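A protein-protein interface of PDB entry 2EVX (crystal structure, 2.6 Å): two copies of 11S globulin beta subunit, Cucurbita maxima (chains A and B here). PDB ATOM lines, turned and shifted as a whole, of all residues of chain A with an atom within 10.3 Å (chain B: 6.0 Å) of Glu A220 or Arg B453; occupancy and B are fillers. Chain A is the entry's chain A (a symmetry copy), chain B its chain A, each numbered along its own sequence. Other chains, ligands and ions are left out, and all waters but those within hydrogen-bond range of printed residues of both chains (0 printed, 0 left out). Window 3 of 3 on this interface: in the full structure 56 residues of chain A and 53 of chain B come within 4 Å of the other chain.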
ATOM      1  N   PHE A 213       2.364  -8.257  15.959  1.00  0.00           N
ATOM      2  CA  PHE A 213       2.404  -7.640  17.282  1.00  0.00           C
ATOM      3  C   PHE A 213       3.801  -7.425  17.848  1.00  0.00           C
ATOM      4  O   PHE A 213       4.723  -8.203  17.593  1.00  0.00           O
ATOM      5  CB  PHE A 213       1.596  -8.474  18.285  1.00  0.00           C
ATOM      6  CG  PHE A 213       0.109  -8.342  18.120  1.00  0.00           C
ATOM      7  CD1 PHE A 213      -0.506  -7.098  18.228  1.00  0.00           C
ATOM      8  CD2 PHE A 213      -0.672  -9.450  17.834  1.00  0.00           C
ATOM      9  CE1 PHE A 213      -1.863  -6.961  18.053  1.00  0.00           C
ATOM     10  CE2 PHE A 213      -2.030  -9.321  17.658  1.00  0.00           C
ATOM     11  CZ  PHE A 213      -2.626  -8.073  17.767  1.00  0.00           C
ATOM     12  N   ALA A 214       3.927  -6.360  18.636  1.00  0.00           N
ATOM     13  CA  ALA A 214       5.176  -5.981  19.297  1.00  0.00           C
ATOM     14  C   ALA A 214       5.613  -7.017  20.338  1.00  0.00           C
ATOM     15  O   ALA A 214       4.782  -7.543  21.095  1.00  0.00           O
ATOM     16  CB  ALA A 214       5.001  -4.627  19.964  1.00  0.00           C
ATOM     17  N   ASP A 215       6.917  -7.297  20.384  1.00  0.00           N
ATOM     18  CA  ASP A 215       7.453  -8.274  21.328  1.00  0.00           C
ATOM     19  C   ASP A 215       6.968  -8.025  22.759  1.00  0.00           C
ATOM     20  O   ASP A 215       6.507  -8.948  23.439  1.00  0.00           O
ATOM     21  CB  ASP A 215       8.986  -8.274  21.294  1.00  0.00           C
ATOM     22  CG  ASP A 215       9.555  -8.889  20.016  1.00  0.00           C
ATOM     23  OD1 ASP A 215       9.062  -9.948  19.571  1.00  0.00           O
ATOM     24  OD2 ASP A 215      10.519  -8.319  19.463  1.00  0.00           O
ATOM     25  N   GLU A 216       7.067  -6.777  23.208  1.00  0.00           N
ATOM     26  CA  GLU A 216       6.638  -6.412  24.555  1.00  0.00           C
ATOM     27  C   GLU A 216       5.191  -6.847  24.806  1.00  0.00           C
ATOM     28  O   GLU A 216       4.913  -7.615  25.734  1.00  0.00           O
ATOM     29  CB  GLU A 216       6.794  -4.897  24.754  1.00  0.00           C
ATOM     30  CG  GLU A 216       6.194  -4.313  26.044  1.00  0.00           C
ATOM     31  CD  GLU A 216       6.810  -4.859  27.338  1.00  0.00           C
ATOM     32  OE1 GLU A 216       6.618  -4.216  28.397  1.00  0.00           O
ATOM     33  OE2 GLU A 216       7.468  -5.924  27.309  1.00  0.00           O
ATOM     34  N   PHE A 217       4.279  -6.366  23.966  1.00  0.00           N
ATOM     35  CA  PHE A 217       2.864  -6.690  24.085  1.00  0.00           C
ATOM     36  C   PHE A 217       2.606  -8.184  24.244  1.00  0.00           C
ATOM     37  O   PHE A 217       1.833  -8.602  25.105  1.00  0.00           O
ATOM     38  CB  PHE A 217       2.107  -6.177  22.860  1.00  0.00           C
ATOM     39  CG  PHE A 217       1.752  -4.708  22.916  1.00  0.00           C
ATOM     40  CD1 PHE A 217       2.340  -3.860  23.848  1.00  0.00           C
ATOM     41  CD2 PHE A 217       0.814  -4.180  22.033  1.00  0.00           C
ATOM     42  CE1 PHE A 217       1.994  -2.501  23.904  1.00  0.00           C
ATOM     43  CE2 PHE A 217       0.462  -2.829  22.077  1.00  0.00           C
ATOM     44  CZ  PHE A 217       1.055  -1.987  23.018  1.00  0.00           C
ATOM     45  N   LEU A 218       3.252  -8.996  23.419  1.00  0.00           N
ATOM     46  CA  LEU A 218       3.030 -10.431  23.499  1.00  0.00           C
ATOM     47  C   LEU A 218       3.619 -11.079  24.737  1.00  0.00           C
ATOM     48  O   LEU A 218       3.105 -12.095  25.204  1.00  0.00           O
ATOM     49  CB  LEU A 218       3.570 -11.133  22.254  1.00  0.00           C
ATOM     50  CG  LEU A 218       2.854 -10.858  20.929  1.00  0.00           C
ATOM     51  CD1 LEU A 218       3.456 -11.755  19.870  1.00  0.00           C
ATOM     52  CD2 LEU A 218       1.349 -11.118  21.046  1.00  0.00           C
ATOM     53  N   GLU A 219       4.693 -10.501  25.272  1.00  0.00           N
ATOM     54  CA  GLU A 219       5.340 -11.057  26.461  1.00  0.00           C
ATOM     55  C   GLU A 219       4.456 -10.872  27.687  1.00  0.00           C
ATOM     56  O   GLU A 219       4.461 -11.706  28.598  1.00  0.00           O
ATOM     57  CB  GLU A 219       6.702 -10.396  26.693  1.00  0.00           C
ATOM     58  CG  GLU A 219       7.672 -10.570  25.521  1.00  0.00           C
ATOM     59  CD  GLU A 219       8.999  -9.838  25.707  1.00  0.00           C
ATOM     60  OE1 GLU A 219       8.984  -8.669  26.146  1.00  0.00           O
ATOM     61  OE2 GLU A 219      10.056 -10.429  25.395  1.00  0.00           O
ATOM     62  N   GLU A 220       3.692  -9.783  27.697  1.00  0.00           N
ATOM     63  CA  GLU A 220       2.791  -9.491  28.803  1.00  0.00           C
ATOM     64  C   GLU A 220       1.523 -10.332  28.720  1.00  0.00           C
ATOM     65  O   GLU A 220       1.194 -11.080  29.642  1.00  0.00           O
ATOM     66  CB  GLU A 220       2.436  -7.997  28.806  1.00  0.00           C
ATOM     67  CG  GLU A 220       1.685  -7.513  30.052  1.00  0.00           C
ATOM     68  CD  GLU A 220       0.204  -7.882  30.068  1.00  0.00           C
ATOM     69  OE1 GLU A 220      -0.427  -7.712  31.133  1.00  0.00           O
ATOM     70  OE2 GLU A 220      -0.339  -8.325  29.033  1.00  0.00           O
ATOM     71  N   ALA A 221       0.808 -10.184  27.612  1.00  0.00           N
ATOM     72  CA  ALA A 221      -0.428 -10.914  27.390  1.00  0.00           C
ATOM     73  C   ALA A 221      -0.298 -12.375  27.802  1.00  0.00           C
ATOM     74  O   ALA A 221      -1.168 -12.916  28.490  1.00  0.00           O
ATOM     75  CB  ALA A 221      -0.824 -10.821  25.925  1.00  0.00           C
ATOM     76  N   PHE A 222       0.794 -13.010  27.388  1.00  0.00           N
ATOM     77  CA  PHE A 222       1.009 -14.412  27.705  1.00  0.00           C
ATOM     78  C   PHE A 222       1.873 -14.655  28.930  1.00  0.00           C
ATOM     79  O   PHE A 222       1.869 -15.759  29.473  1.00  0.00           O
ATOM     80  CB  PHE A 222       1.644 -15.139  26.517  1.00  0.00           C
ATOM     81  CG  PHE A 222       0.820 -15.103  25.272  1.00  0.00           C
ATOM     82  CD1 PHE A 222       0.751 -13.950  24.502  1.00  0.00           C
ATOM     83  CD2 PHE A 222       0.106 -16.225  24.868  1.00  0.00           C
ATOM     84  CE1 PHE A 222      -0.010 -13.915  23.349  1.00  0.00           C
ATOM     85  CE2 PHE A 222      -0.662 -16.197  23.711  1.00  0.00           C
ATOM     86  CZ  PHE A 222      -0.720 -15.042  22.952  1.00  0.00           C
ATOM     87  N   GLN A 223       2.606 -13.636  29.369  1.00  0.00           N
ATOM     88  CA  GLN A 223       3.497 -13.788  30.523  1.00  0.00           C
ATOM     89  C   GLN A 223       4.599 -14.789  30.134  1.00  0.00           C
ATOM     90  O   GLN A 223       4.711 -15.888  30.700  1.00  0.00           O
ATOM     91  CB  GLN A 223       2.716 -14.288  31.752  1.00  0.00           C
ATOM     92  CG  GLN A 223       1.709 -13.279  32.298  1.00  0.00           C
ATOM     93  CD  GLN A 223       2.369 -12.077  32.978  1.00  0.00           C
ATOM     94  OE1 GLN A 223       2.728 -12.137  34.155  1.00  0.00           O
ATOM     95  NE2 GLN A 223       2.534 -10.986  32.233  1.00  0.00           N
ATOM     96  N   ILE A 224       5.403 -14.390  29.147  1.00  0.00           N
ATOM     97  CA  ILE A 224       6.489 -15.224  28.646  1.00  0.00           C
ATOM     98  C   ILE A 224       7.737 -14.427  28.278  1.00  0.00           C
ATOM     99  O   ILE A 224       7.713 -13.195  28.226  1.00  0.00           O
ATOM    100  CB  ILE A 224       6.039 -16.017  27.408  1.00  0.00           C
ATOM    101  CG1 ILE A 224       5.373 -15.068  26.404  1.00  0.00           C
ATOM    102  CG2 ILE A 224       5.090 -17.122  27.824  1.00  0.00           C
ATOM    103  CD1 ILE A 224       4.978 -15.731  25.104  1.00  0.00           C
ATOM    104  N   ASP A 225       8.825 -15.148  28.024  1.00  0.00           N
ATOM    105  CA  ASP A 225      10.103 -14.540  27.648  1.00  0.00           C
ATOM    106  C   ASP A 225      10.116 -14.230  26.153  1.00  0.00           C
ATOM    107  O   ASP A 225       9.328 -14.792  25.393  1.00  0.00           O
ATOM    108  CB  ASP A 225      11.268 -15.495  27.960  1.00  0.00           C
ATOM    109  CG  ASP A 225      11.170 -16.813  27.187  1.00  0.00           C
ATOM    110  OD1 ASP A 225      12.201 -17.497  27.007  1.00  0.00           O
ATOM    111  OD2 ASP A 225      10.052 -17.173  26.762  1.00  0.00           O
ATOM    112  N   GLY A 226      11.024 -13.350  25.737  1.00  0.00           N
ATOM    113  CA  GLY A 226      11.130 -12.996  24.331  1.00  0.00           C
ATOM    114  C   GLY A 226      11.509 -14.174  23.442  1.00  0.00           C
ATOM    115  O   GLY A 226      11.244 -14.170  22.236  1.00  0.00           O
ATOM    116  N   LEU A 228      10.220 -16.937  23.589  1.00  0.00           N
ATOM    117  CA  LEU A 228       8.947 -17.567  23.285  1.00  0.00           C
ATOM    118  C   LEU A 228       8.175 -16.730  22.289  1.00  0.00           C
ATOM    119  O   LEU A 228       7.450 -17.255  21.454  1.00  0.00           O
ATOM    120  CB  LEU A 228       8.123 -17.743  24.555  1.00  0.00           C
ATOM    121  CG  LEU A 228       8.140 -19.161  25.111  1.00  0.00           C
ATOM    122  CD1 LEU A 228       7.256 -19.239  26.349  1.00  0.00           C
ATOM    123  CD2 LEU A 228       7.652 -20.119  24.029  1.00  0.00           C
ATOM    124  N   VAL A 229       8.327 -15.420  22.385  1.00  0.00           N
ATOM    125  CA  VAL A 229       7.643 -14.545  21.461  1.00  0.00           C
ATOM    126  C   VAL A 229       8.199 -14.824  20.076  1.00  0.00           C
ATOM    127  O   VAL A 229       7.501 -14.681  19.079  1.00  0.00           O
ATOM    128  CB  VAL A 229       7.862 -13.086  21.836  1.00  0.00           C
ATOM    129  CG1 VAL A 229       7.277 -12.180  20.777  1.00  0.00           C
ATOM    130  CG2 VAL A 229       7.214 -12.814  23.179  1.00  0.00           C
ATOM    131  N   LEU A 232       6.464 -18.047  18.918  1.00  0.00           N
ATOM    132  CA  LEU A 232       5.081 -17.696  18.684  1.00  0.00           C
ATOM    133  C   LEU A 232       4.960 -17.040  17.314  1.00  0.00           C
ATOM    134  O   LEU A 232       4.218 -17.509  16.452  1.00  0.00           O
ATOM    135  CB  LEU A 232       4.618 -16.741  19.784  1.00  0.00           C
ATOM    136  CG  LEU A 232       3.122 -16.480  19.967  1.00  0.00           C
ATOM    137  CD1 LEU A 232       2.375 -17.789  20.284  1.00  0.00           C
ATOM    138  CD2 LEU A 232       2.948 -15.460  21.092  1.00  0.00           C
ATOM    139  N   ASN B 332      -1.810   1.765  32.790  1.00  0.00           N
ATOM    140  CA  ASN B 332      -1.028   0.628  32.311  1.00  0.00           C
ATOM    141  C   ASN B 332      -1.806  -0.683  32.162  1.00  0.00           C
ATOM    142  O   ASN B 332      -1.202  -1.747  31.965  1.00  0.00           O
ATOM    143  CB  ASN B 332       0.179   0.385  33.225  1.00  0.00           C
ATOM    144  CG  ASN B 332       1.110   1.587  33.319  1.00  0.00           C
ATOM    145  OD1 ASN B 332       2.335   1.434  33.275  1.00  0.00           O
ATOM    146  ND2 ASN B 332       0.538   2.786  33.465  1.00  0.00           N
ATOM    147  N   MET B 334      -4.079  -3.475  30.339  1.00  0.00           N
ATOM    148  CA  MET B 334      -4.105  -3.964  28.969  1.00  0.00           C
ATOM    149  C   MET B 334      -5.251  -4.933  28.701  1.00  0.00           C
ATOM    150  O   MET B 334      -5.579  -5.765  29.549  1.00  0.00           O
ATOM    151  CB  MET B 334      -2.769  -4.660  28.655  1.00  0.00           C
ATOM    152  CG  MET B 334      -2.748  -5.477  27.363  1.00  0.00           C
ATOM    153  SD  MET B 334      -1.218  -6.445  27.102  1.00  0.00           S
ATOM    154  CE  MET B 334      -0.206  -5.223  26.242  1.00  0.00           C
ATOM    155  N   ARG B 388      -3.535  -1.179  25.343  1.00  0.00           N
ATOM    156  CA  ARG B 388      -2.817  -0.841  26.553  1.00  0.00           C
ATOM    157  C   ARG B 388      -2.985   0.634  26.856  1.00  0.00           C
ATOM    158  O   ARG B 388      -2.565   1.491  26.080  1.00  0.00           O
ATOM    159  CB  ARG B 388      -1.342  -1.179  26.401  1.00  0.00           C
ATOM    160  CG  ARG B 388      -0.411  -0.153  27.007  1.00  0.00           C
ATOM    161  CD  ARG B 388       0.834  -0.829  27.479  1.00  0.00           C
ATOM    162  NE  ARG B 388       0.543  -1.663  28.636  1.00  0.00           N
ATOM    163  CZ  ARG B 388       1.320  -2.656  29.048  1.00  0.00           C
ATOM    164  NH1 ARG B 388       2.434  -2.939  28.383  1.00  0.00           N
ATOM    165  NH2 ARG B 388       0.993  -3.352  30.133  1.00  0.00           N
ATOM    166  N   GLN B 443      -0.801 -17.328  31.530  1.00  0.00           N
ATOM    167  CA  GLN B 443      -1.701 -16.192  31.724  1.00  0.00           C
ATOM    168  C   GLN B 443      -2.876 -16.575  32.618  1.00  0.00           C
ATOM    169  O   GLN B 443      -3.740 -17.373  32.233  1.00  0.00           O
ATOM    170  CB  GLN B 443      -2.206 -15.677  30.372  1.00  0.00           C
ATOM    171  CG  GLN B 443      -3.067 -14.422  30.451  1.00  0.00           C
ATOM    172  CD  GLN B 443      -2.492 -13.373  31.379  1.00  0.00           C
ATOM    173  OE1 GLN B 443      -2.648 -13.458  32.592  1.00  0.00           O
ATOM    174  NE2 GLN B 443      -1.816 -12.386  30.814  1.00  0.00           N
ATOM    175  N   LEU B 449      -6.386  -7.317  31.533  1.00  0.00           N
ATOM    176  CA  LEU B 449      -5.221  -7.723  32.301  1.00  0.00           C
ATOM    177  C   LEU B 449      -4.752  -6.579  33.188  1.00  0.00           C
ATOM    178  O   LEU B 449      -4.590  -5.446  32.738  1.00  0.00           O
ATOM    179  CB  LEU B 449      -4.093  -8.143  31.356  1.00  0.00           C
ATOM    180  CG  LEU B 449      -4.486  -9.151  30.271  1.00  0.00           C
ATOM    181  CD1 LEU B 449      -3.255  -9.576  29.501  1.00  0.00           C
ATOM    182  CD2 LEU B 449      -5.150 -10.364  30.890  1.00  0.00           C
ATOM    183  N   SER B 450      -4.551  -6.877  34.465  1.00  0.00           N
ATOM    184  CA  SER B 450      -4.090  -5.876  35.412  1.00  0.00           C
ATOM    185  C   SER B 450      -2.603  -5.663  35.171  1.00  0.00           C
ATOM    186  O   SER B 450      -1.869  -6.621  34.930  1.00  0.00           O
ATOM    187  CB  SER B 450      -4.335  -6.359  36.844  1.00  0.00           C
ATOM    188  OG  SER B 450      -3.774  -7.644  37.062  1.00  0.00           O
ATOM    189  N   PRO B 451      -2.145  -4.404  35.219  1.00  0.00           N
ATOM    190  CA  PRO B 451      -0.737  -4.062  35.007  1.00  0.00           C
ATOM    191  C   PRO B 451       0.243  -5.174  35.384  1.00  0.00           C
ATOM    192  O   PRO B 451       0.688  -5.286  36.531  1.00  0.00           O
ATOM    193  CB  PRO B 451      -0.574  -2.805  35.851  1.00  0.00           C
ATOM    194  CG  PRO B 451      -1.865  -2.095  35.573  1.00  0.00           C
ATOM    195  CD  PRO B 451      -2.906  -3.218  35.655  1.00  0.00           C
ATOM    196  N   GLY B 452       0.552  -6.006  34.395  1.00  0.00           N
ATOM    197  CA  GLY B 452       1.480  -7.106  34.576  1.00  0.00           C
ATOM    198  C   GLY B 452       2.472  -7.022  33.433  1.00  0.00           C
ATOM    199  O   GLY B 452       2.966  -8.042  32.936  1.00  0.00           O
ATOM    200  N   ARG B 453       2.748  -5.783  33.025  1.00  0.00           N
ATOM    201  CA  ARG B 453       3.666  -5.450  31.930  1.00  0.00           C
ATOM    202  C   ARG B 453       5.079  -6.034  32.049  1.00  0.00           C
ATOM    203  O   ARG B 453       5.912  -5.442  32.776  1.00  0.00           O
ATOM    204  CB  ARG B 453       3.749  -3.924  31.787  1.00  0.00           C
ATOM    205  CG  ARG B 453       4.056  -3.178  33.089  1.00  0.00           C
ATOM    206  CD  ARG B 453       4.153  -1.671  32.866  1.00  0.00           C
ATOM    207  NE  ARG B 453       5.037  -1.339  31.746  1.00  0.00           N
ATOM    208  CZ  ARG B 453       4.622  -1.090  30.504  1.00  0.00           C
ATOM    209  NH1 ARG B 453       3.325  -1.124  30.214  1.00  0.00           N
ATOM    210  NH2 ARG B 453       5.505  -0.818  29.547  1.00  0.00           N
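Printed residues of chain A within 4 Å of Arg B453: Glu A216 (3.8 Å) and Glu A220 (3.4 Å).
Of the printed residues of chain A, Met B334 touches Phe A217 (3.8 Å) and Glu A220 (2.8 Å).
Of the printed residues of chain B, Gln A223 touches Gln B443 (3.9 Å) and Gly B452 (3.1 Å).
Printed residues of chain B within 4 Å of Phe A222: Gln B443.
Printed residues of chain A within 4 Å of Gln B443: Glu A220, Ala A221, Phe A222 and Gln A223.
Val A229 touches none of the printed residues of chain B.
Asp A225 touches none of the printed residues of chain B.
The nearest printed residue of chain B that does not touch Glu A220 is Ser B450 (4.2 Å).
Among the printed residues, pairs that only touch across the chains: Phe A217 with Met B334 (3.8 Å), Glu A220 with Leu B449 (3.2 Å), Glu A220 with Gly B452 (3.2 Å), Glu A220 with Arg B453 (3.4 Å), Ala A221 with Leu B449 (3.8 Å), Phe A222 with Gln B443 (3.7 Å) and Gln A223 with Gln B443 (3.9 Å).
Of the 9 printed residues of chain B, 5 touch a printed residue of chain A.
Printed residues of chain B that touch a printed residue of chain A: Met B334, Gln B443, Leu B449, Gly B452 and Arg B453.
Hydrophobic or aromatic side chains of chain B within 4 Å of the printed part of chain A: Met B334 and Leu B449.
Hydrophobic or aromatic side chains of chain A that line the printed part of chain B: Phe A217.
Along chain A the printed residues that touch a printed residue of chain B span positions 216 to 223.
Among the printed residues, Asp or Glu carboxylates within 4 Å of a Lys or Arg side-chain nitrogen of the other chain: Glu A216 with Arg B453.
NE2 of Gln B443 is in hydrogen-bond range of O of Glu A220 (3.5 Å).
NE2 of Gln B443 lies within hydrogen-bond range of O of Ala A221 (2.5 Å).
SD of Met B334 lies close to OE2 of Glu A220.
The side-chain carboxylate (OE1) of Glu A216 is in salt-bridge range of the guanidinium group (NH2) of Arg B453 (3.8 Å).
O of Gly B452 lies within hydrogen-bond range of NE2 of Gln A223 (3.1 Å).
The guanidinium group (NH1) of Arg B388 lies close to the guanidinium group (NH1) of Arg B453, 2.7 Å away.
The backbone NH (N) of Leu B449 is in hydrogen-bond range of the backbone carbonyl oxygen (O) of Met B334 (2.6 Å).
The backbone carbonyl oxygen (O) of Glu A220 lies within hydrogen-bond range of the side-chain amide nitrogen (NE2) of Gln A223 (2.9 Å).
No position is printed for both chains.
Of the 12 pairs that touch across the chains among the printed residues, none has its exchanged pair printed and touching as well.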
